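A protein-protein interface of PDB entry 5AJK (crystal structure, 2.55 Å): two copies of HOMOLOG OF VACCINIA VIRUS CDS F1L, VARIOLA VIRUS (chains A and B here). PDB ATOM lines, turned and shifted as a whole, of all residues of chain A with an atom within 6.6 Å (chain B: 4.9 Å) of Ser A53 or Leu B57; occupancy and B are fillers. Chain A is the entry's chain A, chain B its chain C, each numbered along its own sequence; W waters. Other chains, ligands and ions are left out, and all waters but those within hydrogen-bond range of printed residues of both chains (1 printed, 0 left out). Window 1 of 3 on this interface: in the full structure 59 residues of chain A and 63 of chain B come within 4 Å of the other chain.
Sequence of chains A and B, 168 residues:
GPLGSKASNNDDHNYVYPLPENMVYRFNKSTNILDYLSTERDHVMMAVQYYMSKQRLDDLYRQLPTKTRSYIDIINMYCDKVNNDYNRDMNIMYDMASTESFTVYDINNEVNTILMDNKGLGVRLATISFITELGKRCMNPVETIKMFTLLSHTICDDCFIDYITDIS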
ATOM      1  N   VAL A  48      27.434  -1.773  20.678  1.00  0.00           N
ATOM      2  CA  VAL A  48      28.461  -0.755  20.483  1.00  0.00           C
ATOM      3  C   VAL A  48      28.132   0.525  21.244  1.00  0.00           C
ATOM      4  O   VAL A  48      29.008   1.125  21.863  1.00  0.00           O
ATOM      5  CB  VAL A  48      28.646  -0.414  18.991  1.00  0.00           C
ATOM      6  CG1 VAL A  48      29.541   0.819  18.817  1.00  0.00           C
ATOM      7  CG2 VAL A  48      29.241  -1.598  18.244  1.00  0.00           C
ATOM      8  N   GLN A  49      26.876   0.951  21.187  1.00  0.00           N
ATOM      9  CA  GLN A  49      26.472   2.183  21.853  1.00  0.00           C
ATOM     10  C   GLN A  49      26.520   2.036  23.363  1.00  0.00           C
ATOM     11  O   GLN A  49      26.849   2.987  24.069  1.00  0.00           O
ATOM     12  CB  GLN A  49      25.071   2.603  21.424  1.00  0.00           C
ATOM     13  CG  GLN A  49      24.994   3.107  20.005  1.00  0.00           C
ATOM     14  CD  GLN A  49      23.632   3.673  19.674  1.00  0.00           C
ATOM     15  OE1 GLN A  49      23.323   4.815  20.014  1.00  0.00           O
ATOM     16  NE2 GLN A  49      22.806   2.874  19.017  1.00  0.00           N
ATOM     17  N   TYR A  50      26.185   0.852  23.862  1.00  0.00           N
ATOM     18  CA  TYR A  50      26.242   0.612  25.298  1.00  0.00           C
ATOM     19  C   TYR A  50      27.692   0.588  25.764  1.00  0.00           C
ATOM     20  O   TYR A  50      28.018   1.109  26.830  1.00  0.00           O
ATOM     21  CB  TYR A  50      25.550  -0.697  25.679  1.00  0.00           C
ATOM     22  CG  TYR A  50      25.593  -0.953  27.167  1.00  0.00           C
ATOM     23  CD1 TYR A  50      24.630  -0.420  28.010  1.00  0.00           C
ATOM     24  CD2 TYR A  50      26.613  -1.705  27.732  1.00  0.00           C
ATOM     25  CE1 TYR A  50      24.674  -0.638  29.371  1.00  0.00           C
ATOM     26  CE2 TYR A  50      26.666  -1.928  29.094  1.00  0.00           C
ATOM     27  CZ  TYR A  50      25.695  -1.392  29.908  1.00  0.00           C
ATOM     28  OH  TYR A  50      25.745  -1.613  31.264  1.00  0.00           O
ATOM     29  N   TYR A  51      28.558  -0.022  24.959  1.00  0.00           N
ATOM     30  CA  TYR A  51      29.982  -0.057  25.260  1.00  0.00           C
ATOM     31  C   TYR A  51      30.537   1.352  25.420  1.00  0.00           C
ATOM     32  O   TYR A  51      31.168   1.670  26.430  1.00  0.00           O
ATOM     33  CB  TYR A  51      30.750  -0.791  24.162  1.00  0.00           C
ATOM     34  CG  TYR A  51      32.250  -0.719  24.338  1.00  0.00           C
ATOM     35  CD1 TYR A  51      32.897  -1.548  25.239  1.00  0.00           C
ATOM     36  CD2 TYR A  51      33.016   0.182  23.610  1.00  0.00           C
ATOM     37  CE1 TYR A  51      34.263  -1.491  25.412  1.00  0.00           C
ATOM     38  CE2 TYR A  51      34.387   0.247  23.773  1.00  0.00           C
ATOM     39  CZ  TYR A  51      35.004  -0.592  24.678  1.00  0.00           C
ATOM     40  OH  TYR A  51      36.368  -0.541  24.855  1.00  0.00           O
ATOM     41  N   MET A  52      30.293   2.191  24.418  1.00  0.00           N
ATOM     42  CA  MET A  52      30.766   3.569  24.443  1.00  0.00           C
ATOM     43  C   MET A  52      30.230   4.311  25.662  1.00  0.00           C
ATOM     44  O   MET A  52      30.973   5.014  26.347  1.00  0.00           O
ATOM     45  CB  MET A  52      30.352   4.302  23.163  1.00  0.00           C
ATOM     46  CG  MET A  52      31.024   3.795  21.892  1.00  0.00           C
ATOM     47  SD  MET A  52      30.400   4.632  20.420  1.00  0.00           S
ATOM     48  CE  MET A  52      31.455   3.930  19.158  1.00  0.00           C
ATOM     49  N   SER A  53      28.940   4.148  25.938  1.00  0.00           N
ATOM     50  CA  SER A  53      28.303   4.877  27.028  1.00  0.00           C
ATOM     51  C   SER A  53      28.750   4.392  28.402  1.00  0.00           C
ATOM     52  O   SER A  53      28.915   5.193  29.317  1.00  0.00           O
ATOM     53  CB  SER A  53      26.787   4.774  26.910  1.00  0.00           C
ATOM     54  OG  SER A  53      26.319   5.642  25.895  1.00  0.00           O
ATOM     55  N   LYS A  54      28.944   3.086  28.544  1.00  0.00           N
ATOM     56  CA  LYS A  54      29.379   2.519  29.815  1.00  0.00           C
ATOM     57  C   LYS A  54      30.833   2.894  30.087  1.00  0.00           C
ATOM     58  O   LYS A  54      31.202   3.215  31.217  1.00  0.00           O
ATOM     59  CB  LYS A  54      29.202   0.998  29.810  1.00  0.00           C
ATOM     60  CG  LYS A  54      29.433   0.318  31.157  1.00  0.00           C
ATOM     61  CD  LYS A  54      28.521   0.883  32.234  1.00  0.00           C
ATOM     62  CE  LYS A  54      28.316  -0.102  33.376  1.00  0.00           C
ATOM     63  NZ  LYS A  54      29.603  -0.612  33.922  1.00  0.00           N
ATOM     64  N   GLN A  55      31.653   2.861  29.041  1.00  0.00           N
ATOM     65  CA  GLN A  55      33.054   3.234  29.156  1.00  0.00           C
ATOM     66  C   GLN A  55      33.187   4.681  29.623  1.00  0.00           C
ATOM     67  O   GLN A  55      33.940   4.973  30.552  1.00  0.00           O
ATOM     68  CB  GLN A  55      33.773   3.039  27.822  1.00  0.00           C
ATOM     69  CG  GLN A  55      34.121   1.594  27.515  1.00  0.00           C
ATOM     70  CD  GLN A  55      35.226   1.063  28.407  1.00  0.00           C
ATOM     71  OE1 GLN A  55      36.314   1.635  28.475  1.00  0.00           O
ATOM     72  NE2 GLN A  55      34.947  -0.034  29.104  1.00  0.00           N
ATOM     73  N   ARG A  56      32.446   5.581  28.983  1.00  0.00           N
ATOM     74  CA  ARG A  56      32.479   6.995  29.343  1.00  0.00           C
ATOM     75  C   ARG A  56      32.006   7.196  30.779  1.00  0.00           C
ATOM     76  O   ARG A  56      32.619   7.946  31.543  1.00  0.00           O
ATOM     77  CB  ARG A  56      31.629   7.811  28.348  1.00  0.00           C
ATOM     78  CG  ARG A  56      30.773   8.961  28.907  1.00  0.00           C
ATOM     79  CD  ARG A  56      31.203  10.305  28.392  1.00  0.00           C
ATOM     80  NE  ARG A  56      30.412  11.365  29.014  1.00  0.00           N
ATOM     81  CZ  ARG A  56      30.625  12.667  28.847  1.00  0.00           C
ATOM     82  NH1 ARG A  56      31.612  13.086  28.069  1.00  0.00           N
ATOM     83  NH2 ARG A  56      29.849  13.546  29.462  1.00  0.00           N
ATOM     84  N   LEU A  57      30.913   6.536  31.140  1.00  0.00           N
ATOM     85  CA  LEU A  57      30.270   6.783  32.426  1.00  0.00           C
ATOM     86  C   LEU A  57      31.113   6.268  33.590  1.00  0.00           C
ATOM     87  O   LEU A  57      31.136   6.878  34.656  1.00  0.00           O
ATOM     88  CB  LEU A  57      28.888   6.139  32.458  1.00  0.00           C
ATOM     89  CG  LEU A  57      27.962   6.604  33.582  1.00  0.00           C
ATOM     90  CD1 LEU A  57      27.625   8.082  33.435  1.00  0.00           C
ATOM     91  CD2 LEU A  57      26.692   5.770  33.598  1.00  0.00           C
ATOM     92  N   ASP A  58      31.793   5.142  33.383  1.00  0.00           N
ATOM     93  CA  ASP A  58      32.710   4.602  34.384  1.00  0.00           C
ATOM     94  C   ASP A  58      33.925   5.519  34.547  1.00  0.00           C
ATOM     95  O   ASP A  58      34.385   5.771  35.662  1.00  0.00           O
ATOM     96  CB  ASP A  58      33.185   3.194  34.001  1.00  0.00           C
ATOM     97  CG  ASP A  58      32.082   2.151  34.075  1.00  0.00           C
ATOM     98  OD1 ASP A  58      31.090   2.356  34.805  1.00  0.00           O
ATOM     99  OD2 ASP A  58      32.225   1.104  33.407  1.00  0.00           O
ATOM    100  N   LYS A 136      14.319   6.416  31.157  1.00  0.00           N
ATOM    101  CA  LYS A 136      14.259   4.973  30.969  1.00  0.00           C
ATOM    102  C   LYS A 136      13.276   4.582  29.861  1.00  0.00           C
ATOM    103  O   LYS A 136      13.493   3.600  29.152  1.00  0.00           O
ATOM    104  CB  LYS A 136      13.869   4.286  32.278  1.00  0.00           C
ATOM    105  CG  LYS A 136      14.882   4.456  33.391  1.00  0.00           C
ATOM    106  CD  LYS A 136      14.429   3.749  34.652  1.00  0.00           C
ATOM    107  CE  LYS A 136      15.423   3.942  35.783  1.00  0.00           C
ATOM    108  NZ  LYS A 136      14.945   3.327  37.053  1.00  0.00           N
ATOM    109  N   SER B  53      21.731   9.413  34.378  1.00  0.00           N
ATOM    110  CA  SER B  53      22.416   8.655  33.339  1.00  0.00           C
ATOM    111  C   SER B  53      22.810   7.266  33.833  1.00  0.00           C
ATOM    112  O   SER B  53      22.813   6.307  33.061  1.00  0.00           O
ATOM    113  CB  SER B  53      23.653   9.411  32.848  1.00  0.00           C
ATOM    114  OG  SER B  53      23.292  10.661  32.283  1.00  0.00           O
ATOM    115  N   LYS B  54      23.136   7.156  35.117  1.00  0.00           N
ATOM    116  CA  LYS B  54      23.502   5.866  35.692  1.00  0.00           C
ATOM    117  C   LYS B  54      22.265   4.987  35.804  1.00  0.00           C
ATOM    118  O   LYS B  54      22.308   3.795  35.500  1.00  0.00           O
ATOM    119  CB  LYS B  54      24.157   6.037  37.066  1.00  0.00           C
ATOM    120  CG  LYS B  54      24.631   4.736  37.704  1.00  0.00           C
ATOM    121  CD  LYS B  54      25.844   4.172  36.980  1.00  0.00           C
ATOM    122  CE  LYS B  54      26.082   2.709  37.316  1.00  0.00           C
ATOM    123  NZ  LYS B  54      26.051   2.438  38.780  1.00  0.00           N
ATOM    124  N   GLN B  55      21.168   5.586  36.250  1.00  0.00           N
ATOM    125  CA  GLN B  55      19.899   4.879  36.376  1.00  0.00           C
ATOM    126  C   GLN B  55      19.442   4.323  35.032  1.00  0.00           C
ATOM    127  O   GLN B  55      18.990   3.182  34.945  1.00  0.00           O
ATOM    128  CB  GLN B  55      18.826   5.806  36.946  1.00  0.00           C
ATOM    129  CG  GLN B  55      18.913   6.005  38.446  1.00  0.00           C
ATOM    130  CD  GLN B  55      18.313   4.848  39.221  1.00  0.00           C
ATOM    131  OE1 GLN B  55      17.177   4.445  38.973  1.00  0.00           O
ATOM    132  NE2 GLN B  55      19.076   4.309  40.165  1.00  0.00           N
ATOM    133  N   ARG B  56      19.570   5.131  33.988  1.00  0.00           N
ATOM    134  CA  ARG B  56      19.105   4.742  32.664  1.00  0.00           C
ATOM    135  C   ARG B  56      19.948   3.621  32.079  1.00  0.00           C
ATOM    136  O   ARG B  56      19.419   2.671  31.502  1.00  0.00           O
ATOM    137  CB  ARG B  56      19.120   5.941  31.719  1.00  0.00           C
ATOM    138  CG  ARG B  56      19.129   5.563  30.244  1.00  0.00           C
ATOM    139  CD  ARG B  56      18.775   6.743  29.375  1.00  0.00           C
ATOM    140  NE  ARG B  56      19.048   6.482  27.963  1.00  0.00           N
ATOM    141  CZ  ARG B  56      18.240   5.809  27.147  1.00  0.00           C
ATOM    142  NH1 ARG B  56      17.093   5.311  27.592  1.00  0.00           N
ATOM    143  NH2 ARG B  56      18.586   5.631  25.879  1.00  0.00           N
ATOM    144  N   LEU B  57      21.261   3.738  32.223  1.00  0.00           N
ATOM    145  CA  LEU B  57      22.171   2.785  31.610  1.00  0.00           C
ATOM    146  C   LEU B  57      22.053   1.425  32.286  1.00  0.00           C
ATOM    147  O   LEU B  57      22.230   0.391  31.645  1.00  0.00           O
ATOM    148  CB  LEU B  57      23.606   3.301  31.685  1.00  0.00           C
ATOM    149  CG  LEU B  57      24.632   2.630  30.773  1.00  0.00           C
ATOM    150  CD1 LEU B  57      24.284   2.847  29.307  1.00  0.00           C
ATOM    151  CD2 LEU B  57      26.027   3.161  31.071  1.00  0.00           C
ATOM    152  N   ASP B  58      21.751   1.430  33.580  1.00  0.00           N
ATOM    153  CA  ASP B  58      21.545   0.190  34.319  1.00  0.00           C
ATOM    154  C   ASP B  58      20.241  -0.455  33.897  1.00  0.00           C
ATOM    155  O   ASP B  58      20.183  -1.657  33.635  1.00  0.00           O
ATOM    156  CB  ASP B  58      21.529   0.445  35.826  1.00  0.00           C
ATOM    157  CG  ASP B  58      22.869   0.913  36.355  1.00  0.00           C
ATOM    158  OD1 ASP B  58      23.897   0.637  35.704  1.00  0.00           O
ATOM    159  OD2 ASP B  58      22.890   1.552  37.429  1.00  0.00           O
ATOM    160  N   ASP B  59      19.192   0.356  33.841  1.00  0.00           N
ATOM    161  CA  ASP B  59      17.882  -0.121  33.439  1.00  0.00           C
ATOM    162  C   ASP B  59      17.925  -0.661  32.019  1.00  0.00           C
ATOM    163  O   ASP B  59      17.252  -1.641  31.696  1.00  0.00           O
ATOM    164  CB  ASP B  59      16.850   0.997  33.543  1.00  0.00           C
ATOM    165  CG  ASP B  59      15.505   0.593  32.987  1.00  0.00           C
ATOM    166  OD1 ASP B  59      14.748  -0.090  33.708  1.00  0.00           O
ATOM    167  OD2 ASP B  59      15.209   0.949  31.827  1.00  0.00           O
ATOM    168  N   LEU B  60      18.722  -0.016  31.174  1.00  0.00           N
ATOM    169  CA  LEU B  60      18.857  -0.448  29.793  1.00  0.00           C
ATOM    170  C   LEU B  60      19.487  -1.832  29.749  1.00  0.00           C
ATOM    171  O   LEU B  60      18.959  -2.741  29.107  1.00  0.00           O
ATOM    172  CB  LEU B  60      19.696   0.547  28.990  1.00  0.00           C
ATOM    173  CG  LEU B  60      20.002   0.153  27.542  1.00  0.00           C
ATOM    174  CD1 LEU B  60      18.718  -0.144  26.767  1.00  0.00           C
ATOM    175  CD2 LEU B  60      20.804   1.242  26.847  1.00  0.00           C
ATOM    176  N   TYR B  61      20.607  -1.990  30.449  1.00  0.00           N
ATOM    177  CA  TYR B  61      21.331  -3.257  30.451  1.00  0.00           C
ATOM    178  C   TYR B  61      20.473  -4.362  31.052  1.00  0.00           C
ATOM    179  O   TYR B  61      20.556  -5.521  30.644  1.00  0.00           O
ATOM    180  CB  TYR B  61      22.648  -3.138  31.227  1.00  0.00           C
ATOM    181  CG  TYR B  61      23.503  -4.379  31.111  1.00  0.00           C
ATOM    182  CD1 TYR B  61      24.315  -4.582  30.003  1.00  0.00           C
ATOM    183  CD2 TYR B  61      23.480  -5.359  32.094  1.00  0.00           C
ATOM    184  CE1 TYR B  61      25.088  -5.719  29.883  1.00  0.00           C
ATOM    185  CE2 TYR B  61      24.249  -6.500  31.983  1.00  0.00           C
ATOM    186  CZ  TYR B  61      25.051  -6.675  30.874  1.00  0.00           C
ATOM    187  OH  TYR B  61      25.821  -7.809  30.757  1.00  0.00           O
ATOM    188  N   PHE B 148      28.579   9.252  19.746  1.00  0.00           N
ATOM    189  CA  PHE B 148      28.360   7.821  19.942  1.00  0.00           C
ATOM    190  C   PHE B 148      27.211   7.319  19.070  1.00  0.00           C
ATOM    191  O   PHE B 148      27.339   6.305  18.383  1.00  0.00           O
ATOM    192  CB  PHE B 148      28.062   7.509  21.415  1.00  0.00           C
ATOM    193  CG  PHE B 148      29.239   7.704  22.345  1.00  0.00           C
ATOM    194  CD1 PHE B 148      30.530   7.832  21.851  1.00  0.00           C
ATOM    195  CD2 PHE B 148      29.050   7.748  23.719  1.00  0.00           C
ATOM    196  CE1 PHE B 148      31.607   8.005  22.711  1.00  0.00           C
ATOM    197  CE2 PHE B 148      30.123   7.921  24.583  1.00  0.00           C
ATOM    198  CZ  PHE B 148      31.401   8.049  24.076  1.00  0.00           C
HETATM  199  O   HOH W   1      16.614   3.161  29.019  1.00  0.00           O
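The side-chain amide oxygen (OE1) of Gln B55 is in hydrogen-bond range of the side-chain amino group (NZ) of Lys A136, 3.1 Å away.
O of Gln A49 sits at hydrogen-bond distance from OG of Ser A53 (3.3 Å). NZ of Lys A54 is in salt-bridge range of OD2 of Asp A58. The side-chain carboxylate (OD2) of Asp B58 lies within salt-bridge range of the side-chain amino group (NZ) of Lys B54, at 3.5 Å.
Leu B57 touches Tyr A50 (O to CE1, 3.5 Å). Tyr A50 touches Tyr B61. Met A52 touches Phe B148. CD2 of Leu B57 touches O of Ser A53, 3.9 Å away. CD of Lys A54 touches CD2 of Leu B57 (3.6 Å). CD2 of Leu A57 touches O of Ser B53, 3.95 Å away. Leu A57 touches Lys B54. Leu A57 touches Leu B57. Asp B59 touches Lys A136.
Ser A53 touches one residue of chain B. Leu B57 touches just these residues of chain A: Tyr A50 (3.5 Å), Ser A53 (3.9 Å), Lys A54 (3.6 Å) and Leu A57 (3.7 Å). Printed residues of chain A within 4 Å of Gln B55: Lys A136. Printed residues of chain A within 4 Å of Lys B54: Leu A57 (3.8 Å). Of the printed residues of chain B, Met A52 touches Phe B148 (3.5 Å). Printed residues of chain B within 4 Å of Leu A57: Ser B53, Lys B54 and Leu B57. The nearest printed residue of chain A that does not touch Gln B55 is Leu A57 (6.1 Å).
Hydrophobic or aromatic side chains of chain B within 4 Å of the printed part of chain A: Leu B57, Tyr B61 and Phe B148. Among the printed residues, 10 pairs touch across the chains. Among the printed residues, no Asp or Glu carboxylate lies within 4 Å of a Lys or Arg side-chain nitrogen of the other chain.
Ser A53 touches Leu B57, and with the chains exchanged Leu A57 touches Ser B53. Lys A54 touches Leu B57, and with the chains exchanged Leu A57 touches Lys B54. Leu B57 touches its own counterpart, Leu A57. Positions printed for both chains: 53, 54, 55, 56, 57 and 58. Of the 10 pairs that touch across the chains among the printed residues, 5 have their exchanged pair printed and touching as well.
Water W1 bridges NH1 of Arg B56 (2.6 Å) and O of Lys A136 (3.2 Å).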
